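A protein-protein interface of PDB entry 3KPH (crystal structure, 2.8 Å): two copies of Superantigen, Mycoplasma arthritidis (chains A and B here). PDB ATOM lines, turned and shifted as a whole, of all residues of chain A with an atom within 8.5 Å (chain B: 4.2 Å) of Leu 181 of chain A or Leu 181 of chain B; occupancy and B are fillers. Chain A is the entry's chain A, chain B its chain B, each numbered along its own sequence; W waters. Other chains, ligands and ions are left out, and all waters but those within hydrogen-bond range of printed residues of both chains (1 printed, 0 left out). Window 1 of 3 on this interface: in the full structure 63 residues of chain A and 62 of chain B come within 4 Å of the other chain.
N of Val 178 of chain A sits at hydrogen-bond distance from OD1 of Asp 175 of chain A (3.2 Å).
The side-chain amino group (NZ) of Lys 176 of chain A is in hydrogen-bond range of the side-chain amide oxygen (OD1) of Asn 177 of chain A, at 3.2 Å.
OD1 of Asp 175 of chain A sits at hydrogen-bond distance from N of Asn 177 of chain A (2.8 Å).
Printed residues of chain B within 4 Å of Leu 136 of chain A: Glu 180, Trp 183 and Phe 184.
Printed residues of chain B within 4 Å of Ile 165 of chain A: Leu 188.
Printed residues of chain B within 4 Å of Leu 181 of chain A: Leu 181 (3.9 Å) and Phe 184 (3.4 Å).
Of chain A, only Leu 181 (3.9 Å) and Phe 184 (3.7 Å) come within 4 Å of Leu 181 of chain B.
Printed residues of chain A within 4 Å of Trp 182 of chain B: Gly 73 (3.7 Å).
Printed residues of chain A within 4 Å of Phe 184 of chain B: Leu 136, Asn 177, Val 178 and Leu 181.
The nearest printed residue of chain B that does not touch Leu 181 of chain A is Arg 185 of chain B (4.01 Å).
The nearest residue of chain A that does not touch Leu 181 of chain B is Arg 185 of chain A (4.04 Å).
The nearest printed residue of chain B that does not touch Phe 133 of chain A is Glu 180 of chain B (4.002 Å).
Asn 177 of chain A touches Phe 184 of chain B, and with the chains exchanged Phe 184 of chain A touches Asn 177 of chain B.
Val 178 of chain A touches Phe 184 of chain B, and with the chains exchanged Phe 184 of chain A touches Val 178 of chain B.
Leu 181 of chain A touches its own counterpart, Leu 181 of chain B.
Leu 181 of chain A touches Phe 184 of chain B, and with the chains exchanged Phe 184 of chain A touches Leu 181 of chain B.
Positions printed for both chains: 177, 178, 179, 180, 181, 182, 183, 184, 185 and 188.
Of the 16 pairs that touch across the chains among the printed residues, 7 have their exchanged pair printed and touching as well.
The backbone carbonyl oxygen (O) of Phe 133 of chain A sits at hydrogen-bond distance from the indole nitrogen (NE1) of Trp 183 of chain B, at 2.9 Å.
Along chain A the printed residues that touch a printed residue of chain B span positions 73 to 184.
Of the 10 printed residues of chain B, 9 touch a printed residue of chain A.
Hydrophobic or aromatic side chains of chain B that line the printed part of chain A: Leu 181, Trp 182, Trp 183, Phe 184 and Leu 188.
Among the printed residues, 16 pairs touch across the chains.
Trp 182 of chain B touches Gly 73 of chain A.
Lys 179 of chain B touches Phe 133 of chain A (O to CZ, 3.99 Å).
Glu 180 of chain B touches Leu 136 of chain A.
Leu 136 of chain A touches Phe 184 of chain B (O to CD1, 3.4 Å).
CD1 of Ile 165 of chain A touches CB of Leu 188 of chain B, 3.9 Å away.
Val 168 of chain A touches Leu 188 of chain B.
Asn 177 of chain A touches Phe 184 of chain B.
Leu 181 of chain A touches Leu 181 of chain B.
Leu 181 of chain A touches Phe 184 of chain B (CD1 to CD2, 3.4 Å).
Leu 181 of chain B touches Phe 184 of chain A (CD1 to CD2, 3.7 Å).
Water W1 lies within hydrogen-bond range of the guanidinium group (NH2) of Arg 185 of chain A (2.7 Å) and the guanidinium group (NE) of Arg 185 of chain B (2.9 Å).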
ATOM      1  N   GLY A  73      15.195  14.313  -9.878  1.00  0.00           N
ATOM      2  CA  GLY A  73      13.817  13.867  -9.913  1.00  0.00           C
ATOM      3  C   GLY A  73      13.562  12.974  -8.722  1.00  0.00           C
ATOM      4  O   GLY A  73      12.418  12.706  -8.365  1.00  0.00           O
ATOM      5  N   PHE A 133      10.386   3.240 -10.855  1.00  0.00           N
ATOM      6  CA  PHE A 133      11.349   4.275 -11.211  1.00  0.00           C
ATOM      7  C   PHE A 133      12.313   3.829 -12.292  1.00  0.00           C
ATOM      8  O   PHE A 133      12.696   4.630 -13.145  1.00  0.00           O
ATOM      9  CB  PHE A 133      12.114   4.755  -9.988  1.00  0.00           C
ATOM     10  CG  PHE A 133      11.433   5.865  -9.264  1.00  0.00           C
ATOM     11  CD1 PHE A 133      10.103   5.743  -8.877  1.00  0.00           C
ATOM     12  CD2 PHE A 133      12.121   7.029  -8.947  1.00  0.00           C
ATOM     13  CE1 PHE A 133       9.469   6.762  -8.180  1.00  0.00           C
ATOM     14  CE2 PHE A 133      11.499   8.053  -8.252  1.00  0.00           C
ATOM     15  CZ  PHE A 133      10.170   7.923  -7.866  1.00  0.00           C
ATOM     16  N   LEU A 136      10.247   3.900 -15.593  1.00  0.00           N
ATOM     17  CA  LEU A 136      10.037   5.247 -16.082  1.00  0.00           C
ATOM     18  C   LEU A 136      11.333   5.850 -16.623  1.00  0.00           C
ATOM     19  O   LEU A 136      11.305   6.587 -17.602  1.00  0.00           O
ATOM     20  CB  LEU A 136       9.437   6.130 -14.982  1.00  0.00           C
ATOM     21  CG  LEU A 136       8.030   5.773 -14.490  1.00  0.00           C
ATOM     22  CD1 LEU A 136       7.668   6.628 -13.308  1.00  0.00           C
ATOM     23  CD2 LEU A 136       7.033   5.986 -15.588  1.00  0.00           C
ATOM     24  N   ILE A 165       7.150  19.968 -21.279  1.00  0.00           N
ATOM     25  CA  ILE A 165       6.258  18.832 -21.099  1.00  0.00           C
ATOM     26  C   ILE A 165       5.131  18.835 -22.135  1.00  0.00           C
ATOM     27  O   ILE A 165       4.681  17.774 -22.564  1.00  0.00           O
ATOM     28  CB  ILE A 165       5.702  18.743 -19.640  1.00  0.00           C
ATOM     29  CG1 ILE A 165       5.907  17.330 -19.112  1.00  0.00           C
ATOM     30  CG2 ILE A 165       4.209  19.024 -19.591  1.00  0.00           C
ATOM     31  CD1 ILE A 165       7.330  16.907 -19.113  1.00  0.00           C
ATOM     32  N   ASN A 166       4.685  20.023 -22.548  1.00  0.00           N
ATOM     33  CA  ASN A 166       3.642  20.135 -23.570  1.00  0.00           C
ATOM     34  C   ASN A 166       4.137  19.437 -24.824  1.00  0.00           C
ATOM     35  O   ASN A 166       3.399  18.713 -25.484  1.00  0.00           O
ATOM     36  CB  ASN A 166       3.381  21.599 -23.927  1.00  0.00           C
ATOM     37  CG  ASN A 166       2.236  22.197 -23.151  1.00  0.00           C
ATOM     38  OD1 ASN A 166       1.131  21.647 -23.140  1.00  0.00           O
ATOM     39  ND2 ASN A 166       2.481  23.340 -22.504  1.00  0.00           N
ATOM     40  N   VAL A 168       6.313  17.031 -25.087  1.00  0.00           N
ATOM     41  CA  VAL A 168       6.303  15.588 -24.940  1.00  0.00           C
ATOM     42  C   VAL A 168       4.893  15.038 -25.167  1.00  0.00           C
ATOM     43  O   VAL A 168       4.728  13.996 -25.799  1.00  0.00           O
ATOM     44  CB  VAL A 168       6.845  15.161 -23.558  1.00  0.00           C
ATOM     45  CG1 VAL A 168       6.700  13.652 -23.364  1.00  0.00           C
ATOM     46  CG2 VAL A 168       8.295  15.544 -23.457  1.00  0.00           C
ATOM     47  N   ARG A 169       3.882  15.744 -24.668  1.00  0.00           N
ATOM     48  CA  ARG A 169       2.497  15.316 -24.834  1.00  0.00           C
ATOM     49  C   ARG A 169       2.145  15.375 -26.317  1.00  0.00           C
ATOM     50  O   ARG A 169       1.564  14.445 -26.868  1.00  0.00           O
ATOM     51  CB  ARG A 169       1.586  16.224 -23.995  1.00  0.00           C
ATOM     52  CG  ARG A 169       0.271  16.652 -24.622  1.00  0.00           C
ATOM     53  CD  ARG A 169      -0.776  15.563 -24.601  1.00  0.00           C
ATOM     54  NE  ARG A 169      -2.097  16.125 -24.880  1.00  0.00           N
ATOM     55  CZ  ARG A 169      -3.244  15.463 -24.738  1.00  0.00           C
ATOM     56  NH1 ARG A 169      -3.238  14.197 -24.322  1.00  0.00           N
ATOM     57  NH2 ARG A 169      -4.401  16.073 -24.989  1.00  0.00           N
ATOM     58  N   ASP A 175       1.478   7.403 -25.858  1.00  0.00           N
ATOM     59  CA  ASP A 175       2.270   6.520 -25.005  1.00  0.00           C
ATOM     60  C   ASP A 175       1.590   6.289 -23.661  1.00  0.00           C
ATOM     61  O   ASP A 175       1.077   7.210 -23.047  1.00  0.00           O
ATOM     62  CB  ASP A 175       3.686   7.093 -24.814  1.00  0.00           C
ATOM     63  CG  ASP A 175       4.563   6.230 -23.905  1.00  0.00           C
ATOM     64  OD1 ASP A 175       4.515   6.409 -22.662  1.00  0.00           O
ATOM     65  OD2 ASP A 175       5.301   5.368 -24.435  1.00  0.00           O
ATOM     66  N   LYS A 176       1.580   5.041 -23.211  1.00  0.00           N
ATOM     67  CA  LYS A 176       0.957   4.692 -21.944  1.00  0.00           C
ATOM     68  C   LYS A 176       1.424   5.552 -20.783  1.00  0.00           C
ATOM     69  O   LYS A 176       0.610   6.045 -20.008  1.00  0.00           O
ATOM     70  CB  LYS A 176       1.240   3.233 -21.599  1.00  0.00           C
ATOM     71  CG  LYS A 176       0.899   2.878 -20.149  1.00  0.00           C
ATOM     72  CD  LYS A 176       1.917   1.903 -19.558  1.00  0.00           C
ATOM     73  CE  LYS A 176       1.914   1.916 -18.015  1.00  0.00           C
ATOM     74  NZ  LYS A 176       3.227   1.465 -17.404  1.00  0.00           N
ATOM     75  N   ASN A 177       2.737   5.724 -20.651  1.00  0.00           N
ATOM     76  CA  ASN A 177       3.286   6.504 -19.542  1.00  0.00           C
ATOM     77  C   ASN A 177       3.053   8.009 -19.626  1.00  0.00           C
ATOM     78  O   ASN A 177       2.641   8.616 -18.637  1.00  0.00           O
ATOM     79  CB  ASN A 177       4.783   6.219 -19.359  1.00  0.00           C
ATOM     80  CG  ASN A 177       5.053   4.803 -18.849  1.00  0.00           C
ATOM     81  OD1 ASN A 177       4.449   4.357 -17.872  1.00  0.00           O
ATOM     82  ND2 ASN A 177       5.971   4.097 -19.505  1.00  0.00           N
ATOM     83  N   VAL A 178       3.308   8.631 -20.773  1.00  0.00           N
ATOM     84  CA  VAL A 178       3.082  10.071 -20.841  1.00  0.00           C
ATOM     85  C   VAL A 178       1.582  10.364 -20.774  1.00  0.00           C
ATOM     86  O   VAL A 178       1.171  11.479 -20.450  1.00  0.00           O
ATOM     87  CB  VAL A 178       3.733  10.713 -22.117  1.00  0.00           C
ATOM     88  CG1 VAL A 178       3.548   9.834 -23.299  1.00  0.00           C
ATOM     89  CG2 VAL A 178       3.124  12.071 -22.405  1.00  0.00           C
ATOM     90  N   LYS A 179       0.776   9.341 -21.049  1.00  0.00           N
ATOM     91  CA  LYS A 179      -0.682   9.454 -21.019  1.00  0.00           C
ATOM     92  C   LYS A 179      -1.090   9.617 -19.550  1.00  0.00           C
ATOM     93  O   LYS A 179      -1.768  10.587 -19.172  1.00  0.00           O
ATOM     94  CB  LYS A 179      -1.298   8.174 -21.603  1.00  0.00           C
ATOM     95  CG  LYS A 179      -2.535   8.386 -22.457  1.00  0.00           C
ATOM     96  CD  LYS A 179      -3.031   7.078 -23.101  1.00  0.00           C
ATOM     97  CE  LYS A 179      -3.193   5.957 -22.068  1.00  0.00           C
ATOM     98  NZ  LYS A 179      -3.864   4.730 -22.619  1.00  0.00           N
ATOM     99  N   GLU A 180      -0.660   8.663 -18.724  1.00  0.00           N
ATOM    100  CA  GLU A 180      -0.965   8.702 -17.301  1.00  0.00           C
ATOM    101  C   GLU A 180      -0.410   9.983 -16.692  1.00  0.00           C
ATOM    102  O   GLU A 180      -1.062  10.613 -15.877  1.00  0.00           O
ATOM    103  CB  GLU A 180      -0.376   7.489 -16.587  1.00  0.00           C
ATOM    104  CG  GLU A 180      -0.790   6.188 -17.215  1.00  0.00           C
ATOM    105  CD  GLU A 180      -0.298   4.953 -16.469  1.00  0.00           C
ATOM    106  OE1 GLU A 180      -0.566   3.825 -16.946  1.00  0.00           O
ATOM    107  OE2 GLU A 180       0.351   5.100 -15.410  1.00  0.00           O
ATOM    108  N   LEU A 181       0.789  10.382 -17.094  1.00  0.00           N
ATOM    109  CA  LEU A 181       1.375  11.591 -16.542  1.00  0.00           C
ATOM    110  C   LEU A 181       0.544  12.804 -16.895  1.00  0.00           C
ATOM    111  O   LEU A 181       0.306  13.661 -16.053  1.00  0.00           O
ATOM    112  CB  LEU A 181       2.804  11.789 -17.055  1.00  0.00           C
ATOM    113  CG  LEU A 181       3.528  13.094 -16.665  1.00  0.00           C
ATOM    114  CD1 LEU A 181       5.002  12.812 -16.554  1.00  0.00           C
ATOM    115  CD2 LEU A 181       3.270  14.209 -17.674  1.00  0.00           C
ATOM    116  N   TRP A 182       0.096  12.887 -18.140  1.00  0.00           N
ATOM    117  CA  TRP A 182      -0.694  14.034 -18.575  1.00  0.00           C
ATOM    118  C   TRP A 182      -2.072  14.109 -17.892  1.00  0.00           C
ATOM    119  O   TRP A 182      -2.547  15.188 -17.532  1.00  0.00           O
ATOM    120  CB  TRP A 182      -0.856  13.977 -20.082  1.00  0.00           C
ATOM    121  CG  TRP A 182      -1.448  15.193 -20.650  1.00  0.00           C
ATOM    122  CD1 TRP A 182      -2.666  15.307 -21.238  1.00  0.00           C
ATOM    123  CD2 TRP A 182      -0.837  16.478 -20.734  1.00  0.00           C
ATOM    124  NE1 TRP A 182      -2.856  16.586 -21.692  1.00  0.00           N
ATOM    125  CE2 TRP A 182      -1.745  17.329 -21.397  1.00  0.00           C
ATOM    126  CE3 TRP A 182       0.394  16.996 -20.314  1.00  0.00           C
ATOM    127  CZ2 TRP A 182      -1.467  18.668 -21.654  1.00  0.00           C
ATOM    128  CZ3 TRP A 182       0.675  18.334 -20.568  1.00  0.00           C
ATOM    129  CH2 TRP A 182      -0.253  19.154 -21.233  1.00  0.00           C
ATOM    130  N   TRP A 183      -2.702  12.955 -17.721  1.00  0.00           N
ATOM    131  CA  TRP A 183      -4.007  12.843 -17.082  1.00  0.00           C
ATOM    132  C   TRP A 183      -3.921  13.299 -15.635  1.00  0.00           C
ATOM    133  O   TRP A 183      -4.585  14.242 -15.219  1.00  0.00           O
ATOM    134  CB  TRP A 183      -4.435  11.380 -17.120  1.00  0.00           C
ATOM    135  CG  TRP A 183      -5.686  11.057 -16.392  1.00  0.00           C
ATOM    136  CD1 TRP A 183      -5.858  10.081 -15.455  1.00  0.00           C
ATOM    137  CD2 TRP A 183      -6.966  11.639 -16.607  1.00  0.00           C
ATOM    138  NE1 TRP A 183      -7.170  10.015 -15.077  1.00  0.00           N
ATOM    139  CE2 TRP A 183      -7.876  10.963 -15.771  1.00  0.00           C
ATOM    140  CE3 TRP A 183      -7.437  12.671 -17.430  1.00  0.00           C
ATOM    141  CZ2 TRP A 183      -9.239  11.284 -15.731  1.00  0.00           C
ATOM    142  CZ3 TRP A 183      -8.792  12.991 -17.392  1.00  0.00           C
ATOM    143  CH2 TRP A 183      -9.676  12.298 -16.549  1.00  0.00           C
ATOM    144  N   PHE A 184      -3.090  12.604 -14.867  1.00  0.00           N
ATOM    145  CA  PHE A 184      -2.895  12.896 -13.457  1.00  0.00           C
ATOM    146  C   PHE A 184      -2.430  14.322 -13.292  1.00  0.00           C
ATOM    147  O   PHE A 184      -2.809  14.995 -12.347  1.00  0.00           O
ATOM    148  CB  PHE A 184      -1.855  11.943 -12.889  1.00  0.00           C
ATOM    149  CG  PHE A 184      -1.677  12.028 -11.404  1.00  0.00           C
ATOM    150  CD1 PHE A 184      -2.769  11.941 -10.551  1.00  0.00           C
ATOM    151  CD2 PHE A 184      -0.398  12.091 -10.852  1.00  0.00           C
ATOM    152  CE1 PHE A 184      -2.586  11.905  -9.159  1.00  0.00           C
ATOM    153  CE2 PHE A 184      -0.208  12.057  -9.476  1.00  0.00           C
ATOM    154  CZ  PHE A 184      -1.302  11.961  -8.625  1.00  0.00           C
ATOM    155  N   ARG A 185      -1.608  14.789 -14.217  1.00  0.00           N
ATOM    156  CA  ARG A 185      -1.108  16.152 -14.128  1.00  0.00           C
ATOM    157  C   ARG A 185      -2.244  17.156 -14.256  1.00  0.00           C
ATOM    158  O   ARG A 185      -2.396  18.043 -13.412  1.00  0.00           O
ATOM    159  CB  ARG A 185      -0.078  16.416 -15.221  1.00  0.00           C
ATOM    160  CG  ARG A 185       0.404  17.847 -15.281  1.00  0.00           C
ATOM    161  CD  ARG A 185       1.340  18.030 -16.458  1.00  0.00           C
ATOM    162  NE  ARG A 185       2.081  19.281 -16.360  1.00  0.00           N
ATOM    163  CZ  ARG A 185       1.539  20.481 -16.525  1.00  0.00           C
ATOM    164  NH1 ARG A 185       0.251  20.584 -16.815  1.00  0.00           N
ATOM    165  NH2 ARG A 185       2.283  21.575 -16.366  1.00  0.00           N
ATOM    166  N   SER A 186      -3.043  17.013 -15.313  1.00  0.00           N
ATOM    167  CA  SER A 186      -4.153  17.923 -15.567  1.00  0.00           C
ATOM    168  C   SER A 186      -5.098  18.031 -14.375  1.00  0.00           C
ATOM    169  O   SER A 186      -5.552  19.125 -14.037  1.00  0.00           O
ATOM    170  CB  SER A 186      -4.924  17.486 -16.813  1.00  0.00           C
ATOM    171  OG  SER A 186      -5.552  16.235 -16.610  1.00  0.00           O
ATOM    172  N   LEU A 187      -5.394  16.905 -13.736  1.00  0.00           N
ATOM    173  CA  LEU A 187      -6.271  16.934 -12.580  1.00  0.00           C
ATOM    174  C   LEU A 187      -5.607  17.668 -11.407  1.00  0.00           C
ATOM    175  O   LEU A 187      -6.223  18.530 -10.785  1.00  0.00           O
ATOM    176  CB  LEU A 187      -6.671  15.512 -12.188  1.00  0.00           C
ATOM    177  CG  LEU A 187      -7.915  14.968 -12.892  1.00  0.00           C
ATOM    178  CD1 LEU A 187      -7.921  15.360 -14.337  1.00  0.00           C
ATOM    179  CD2 LEU A 187      -7.950  13.468 -12.766  1.00  0.00           C
ATOM    180  N   LEU A 188      -4.348  17.351 -11.122  1.00  0.00           N
ATOM    181  CA  LEU A 188      -3.650  17.997 -10.014  1.00  0.00           C
ATOM    182  C   LEU A 188      -3.633  19.506 -10.186  1.00  0.00           C
ATOM    183  O   LEU A 188      -3.942  20.252  -9.255  1.00  0.00           O
ATOM    184  CB  LEU A 188      -2.215  17.476  -9.885  1.00  0.00           C
ATOM    185  CG  LEU A 188      -2.053  16.020  -9.440  1.00  0.00           C
ATOM    186  CD1 LEU A 188      -0.578  15.699  -9.380  1.00  0.00           C
ATOM    187  CD2 LEU A 188      -2.706  15.784  -8.090  1.00  0.00           C
ATOM    188  N   VAL A 189      -3.278  19.966 -11.377  1.00  0.00           N
ATOM    189  CA  VAL A 189      -3.238  21.400 -11.610  1.00  0.00           C
ATOM    190  C   VAL A 189      -4.618  22.020 -11.445  1.00  0.00           C
ATOM    191  O   VAL A 189      -4.757  23.095 -10.873  1.00  0.00           O
ATOM    192  CB  VAL A 189      -2.724  21.709 -12.990  1.00  0.00           C
ATOM    193  CG1 VAL A 189      -2.523  23.191 -13.120  1.00  0.00           C
ATOM    194  CG2 VAL A 189      -1.427  20.948 -13.228  1.00  0.00           C
ATOM    195  N   ASN B 177       2.136   8.366  -6.131  1.00  0.00           N
ATOM    196  CA  ASN B 177       1.790   8.849  -7.451  1.00  0.00           C
ATOM    197  C   ASN B 177       2.450  10.153  -7.851  1.00  0.00           C
ATOM    198  O   ASN B 177       2.955  10.255  -8.968  1.00  0.00           O
ATOM    199  CB  ASN B 177       0.285   8.961  -7.577  1.00  0.00           C
ATOM    200  CG  ASN B 177      -0.375   7.615  -7.651  1.00  0.00           C
ATOM    201  OD1 ASN B 177      -1.272   7.307  -6.874  1.00  0.00           O
ATOM    202  ND2 ASN B 177       0.068   6.794  -8.593  1.00  0.00           N
ATOM    203  N   VAL B 178       2.465  11.156  -6.974  1.00  0.00           N
ATOM    204  CA  VAL B 178       3.106  12.411  -7.373  1.00  0.00           C
ATOM    205  C   VAL B 178       4.629  12.218  -7.454  1.00  0.00           C
ATOM    206  O   VAL B 178       5.337  12.988  -8.122  1.00  0.00           O
ATOM    207  CB  VAL B 178       2.700  13.617  -6.444  1.00  0.00           C
ATOM    208  CG1 VAL B 178       1.745  13.144  -5.367  1.00  0.00           C
ATOM    209  CG2 VAL B 178       3.927  14.310  -5.873  1.00  0.00           C
ATOM    210  N   LYS B 179       5.120  11.163  -6.800  1.00  0.00           N
ATOM    211  CA  LYS B 179       6.548  10.840  -6.834  1.00  0.00           C
ATOM    212  C   LYS B 179       6.882  10.379  -8.243  1.00  0.00           C
ATOM    213  O   LYS B 179       7.765  10.931  -8.895  1.00  0.00           O
ATOM    214  CB  LYS B 179       6.890   9.731  -5.844  1.00  0.00           C
ATOM    215  CG  LYS B 179       7.564  10.230  -4.582  1.00  0.00           C
ATOM    216  CD  LYS B 179       7.993   9.076  -3.689  1.00  0.00           C
ATOM    217  CE  LYS B 179       8.960   9.537  -2.619  1.00  0.00           C
ATOM    218  NZ  LYS B 179       9.367   8.387  -1.765  1.00  0.00           N
ATOM    219  N   GLU B 180       6.159   9.362  -8.709  1.00  0.00           N
ATOM    220  CA  GLU B 180       6.355   8.835 -10.052  1.00  0.00           C
ATOM    221  C   GLU B 180       6.179   9.954 -11.075  1.00  0.00           C
ATOM    222  O   GLU B 180       6.957  10.066 -12.016  1.00  0.00           O
ATOM    223  CB  GLU B 180       5.365   7.699 -10.315  1.00  0.00           C
ATOM    224  CG  GLU B 180       5.789   6.384  -9.706  1.00  0.00           C
ATOM    225  CD  GLU B 180       4.689   5.339  -9.704  1.00  0.00           C
ATOM    226  OE1 GLU B 180       3.837   5.372 -10.615  1.00  0.00           O
ATOM    227  OE2 GLU B 180       4.676   4.470  -8.801  1.00  0.00           O
ATOM    228  N   LEU B 181       5.169  10.794 -10.892  1.00  0.00           N
ATOM    229  CA  LEU B 181       4.952  11.887 -11.824  1.00  0.00           C
ATOM    230  C   LEU B 181       6.125  12.847 -11.850  1.00  0.00           C
ATOM    231  O   LEU B 181       6.555  13.280 -12.911  1.00  0.00           O
ATOM    232  CB  LEU B 181       3.690  12.668 -11.470  1.00  0.00           C
ATOM    233  CG  LEU B 181       3.517  13.905 -12.357  1.00  0.00           C
ATOM    234  CD1 LEU B 181       2.056  14.140 -12.630  1.00  0.00           C
ATOM    235  CD2 LEU B 181       4.153  15.120 -11.690  1.00  0.00           C
ATOM    236  N   TRP B 182       6.650  13.185 -10.682  1.00  0.00           N
ATOM    237  CA  TRP B 182       7.759  14.124 -10.635  1.00  0.00           C
ATOM    238  C   TRP B 182       9.066  13.562 -11.217  1.00  0.00           C
ATOM    239  O   TRP B 182       9.815  14.270 -11.884  1.00  0.00           O
ATOM    240  CB  TRP B 182       7.966  14.608  -9.203  1.00  0.00           C
ATOM    241  CG  TRP B 182       8.899  15.747  -9.136  1.00  0.00           C
ATOM    242  CD1 TRP B 182      10.227  15.695  -8.864  1.00  0.00           C
ATOM    243  CD2 TRP B 182       8.597  17.117  -9.403  1.00  0.00           C
ATOM    244  NE1 TRP B 182      10.782  16.950  -8.944  1.00  0.00           N
ATOM    245  CE2 TRP B 182       9.800  17.843  -9.275  1.00  0.00           C
ATOM    246  CE3 TRP B 182       7.426  17.802  -9.739  1.00  0.00           C
ATOM    247  CZ2 TRP B 182       9.871  19.222  -9.470  1.00  0.00           C
ATOM    248  CZ3 TRP B 182       7.492  19.175  -9.936  1.00  0.00           C
ATOM    249  CH2 TRP B 182       8.711  19.871  -9.801  1.00  0.00           C
ATOM    250  N   TRP B 183       9.325  12.286 -10.962  1.00  0.00           N
ATOM    251  CA  TRP B 183      10.521  11.607 -11.454  1.00  0.00           C
ATOM    252  C   TRP B 183      10.495  11.519 -12.984  1.00  0.00           C
ATOM    253  O   TRP B 183      11.392  12.015 -13.660  1.00  0.00           O
ATOM    254  CB  TRP B 183      10.586  10.215 -10.804  1.00  0.00           C
ATOM    255  CG  TRP B 183      11.503   9.218 -11.432  1.00  0.00           C
ATOM    256  CD1 TRP B 183      11.140   8.117 -12.153  1.00  0.00           C
ATOM    257  CD2 TRP B 183      12.930   9.174 -11.324  1.00  0.00           C
ATOM    258  NE1 TRP B 183      12.250   7.382 -12.493  1.00  0.00           N
ATOM    259  CE2 TRP B 183      13.365   8.007 -11.997  1.00  0.00           C
ATOM    260  CE3 TRP B 183      13.889  10.002 -10.719  1.00  0.00           C
ATOM    261  CZ2 TRP B 183      14.714   7.650 -12.083  1.00  0.00           C
ATOM    262  CZ3 TRP B 183      15.234   9.645 -10.804  1.00  0.00           C
ATOM    263  CH2 TRP B 183      15.630   8.479 -11.481  1.00  0.00           C
ATOM    264  N   PHE B 184       9.450  10.904 -13.524  1.00  0.00           N
ATOM    265  CA  PHE B 184       9.291  10.767 -14.963  1.00  0.00           C
ATOM    266  C   PHE B 184       9.237  12.150 -15.616  1.00  0.00           C
ATOM    267  O   PHE B 184       9.725  12.345 -16.729  1.00  0.00           O
ATOM    268  CB  PHE B 184       8.011   9.976 -15.260  1.00  0.00           C
ATOM    269  CG  PHE B 184       7.825   9.623 -16.711  1.00  0.00           C
ATOM    270  CD1 PHE B 184       8.769   8.865 -17.384  1.00  0.00           C
ATOM    271  CD2 PHE B 184       6.689  10.033 -17.401  1.00  0.00           C
ATOM    272  CE1 PHE B 184       8.582   8.521 -18.723  1.00  0.00           C
ATOM    273  CE2 PHE B 184       6.495   9.692 -18.737  1.00  0.00           C
ATOM    274  CZ  PHE B 184       7.440   8.936 -19.396  1.00  0.00           C
ATOM    275  N   ARG B 185       8.652  13.117 -14.924  1.00  0.00           N
ATOM    276  CA  ARG B 185       8.571  14.457 -15.475  1.00  0.00           C
ATOM    277  C   ARG B 185       9.953  15.057 -15.621  1.00  0.00           C
ATOM    278  O   ARG B 185      10.309  15.545 -16.688  1.00  0.00           O
ATOM    279  CB  ARG B 185       7.719  15.357 -14.577  1.00  0.00           C
ATOM    280  CG  ARG B 185       7.763  16.838 -14.931  1.00  0.00           C
ATOM    281  CD  ARG B 185       6.718  17.585 -14.145  1.00  0.00           C
ATOM    282  NE  ARG B 185       6.713  19.012 -14.431  1.00  0.00           N
ATOM    283  CZ  ARG B 185       7.693  19.845 -14.093  1.00  0.00           C
ATOM    284  NH1 ARG B 185       8.759  19.390 -13.454  1.00  0.00           N
ATOM    285  NH2 ARG B 185       7.605  21.133 -14.394  1.00  0.00           N
ATOM    286  N   LEU B 188      11.854  13.563 -18.535  1.00  0.00           N
ATOM    287  CA  LEU B 188      11.329  14.030 -19.815  1.00  0.00           C
ATOM    288  C   LEU B 188      11.804  15.441 -20.145  1.00  0.00           C
ATOM    289  O   LEU B 188      12.307  15.693 -21.236  1.00  0.00           O
ATOM    290  CB  LEU B 188       9.798  13.991 -19.820  1.00  0.00           C
ATOM    291  CG  LEU B 188       9.172  12.607 -19.998  1.00  0.00           C
ATOM    292  CD1 LEU B 188       7.665  12.662 -19.757  1.00  0.00           C
ATOM    293  CD2 LEU B 188       9.476  12.115 -21.397  1.00  0.00           C
HETATM  294  O   HOH W   1       4.687  20.418 -15.899  1.00  0.00           O
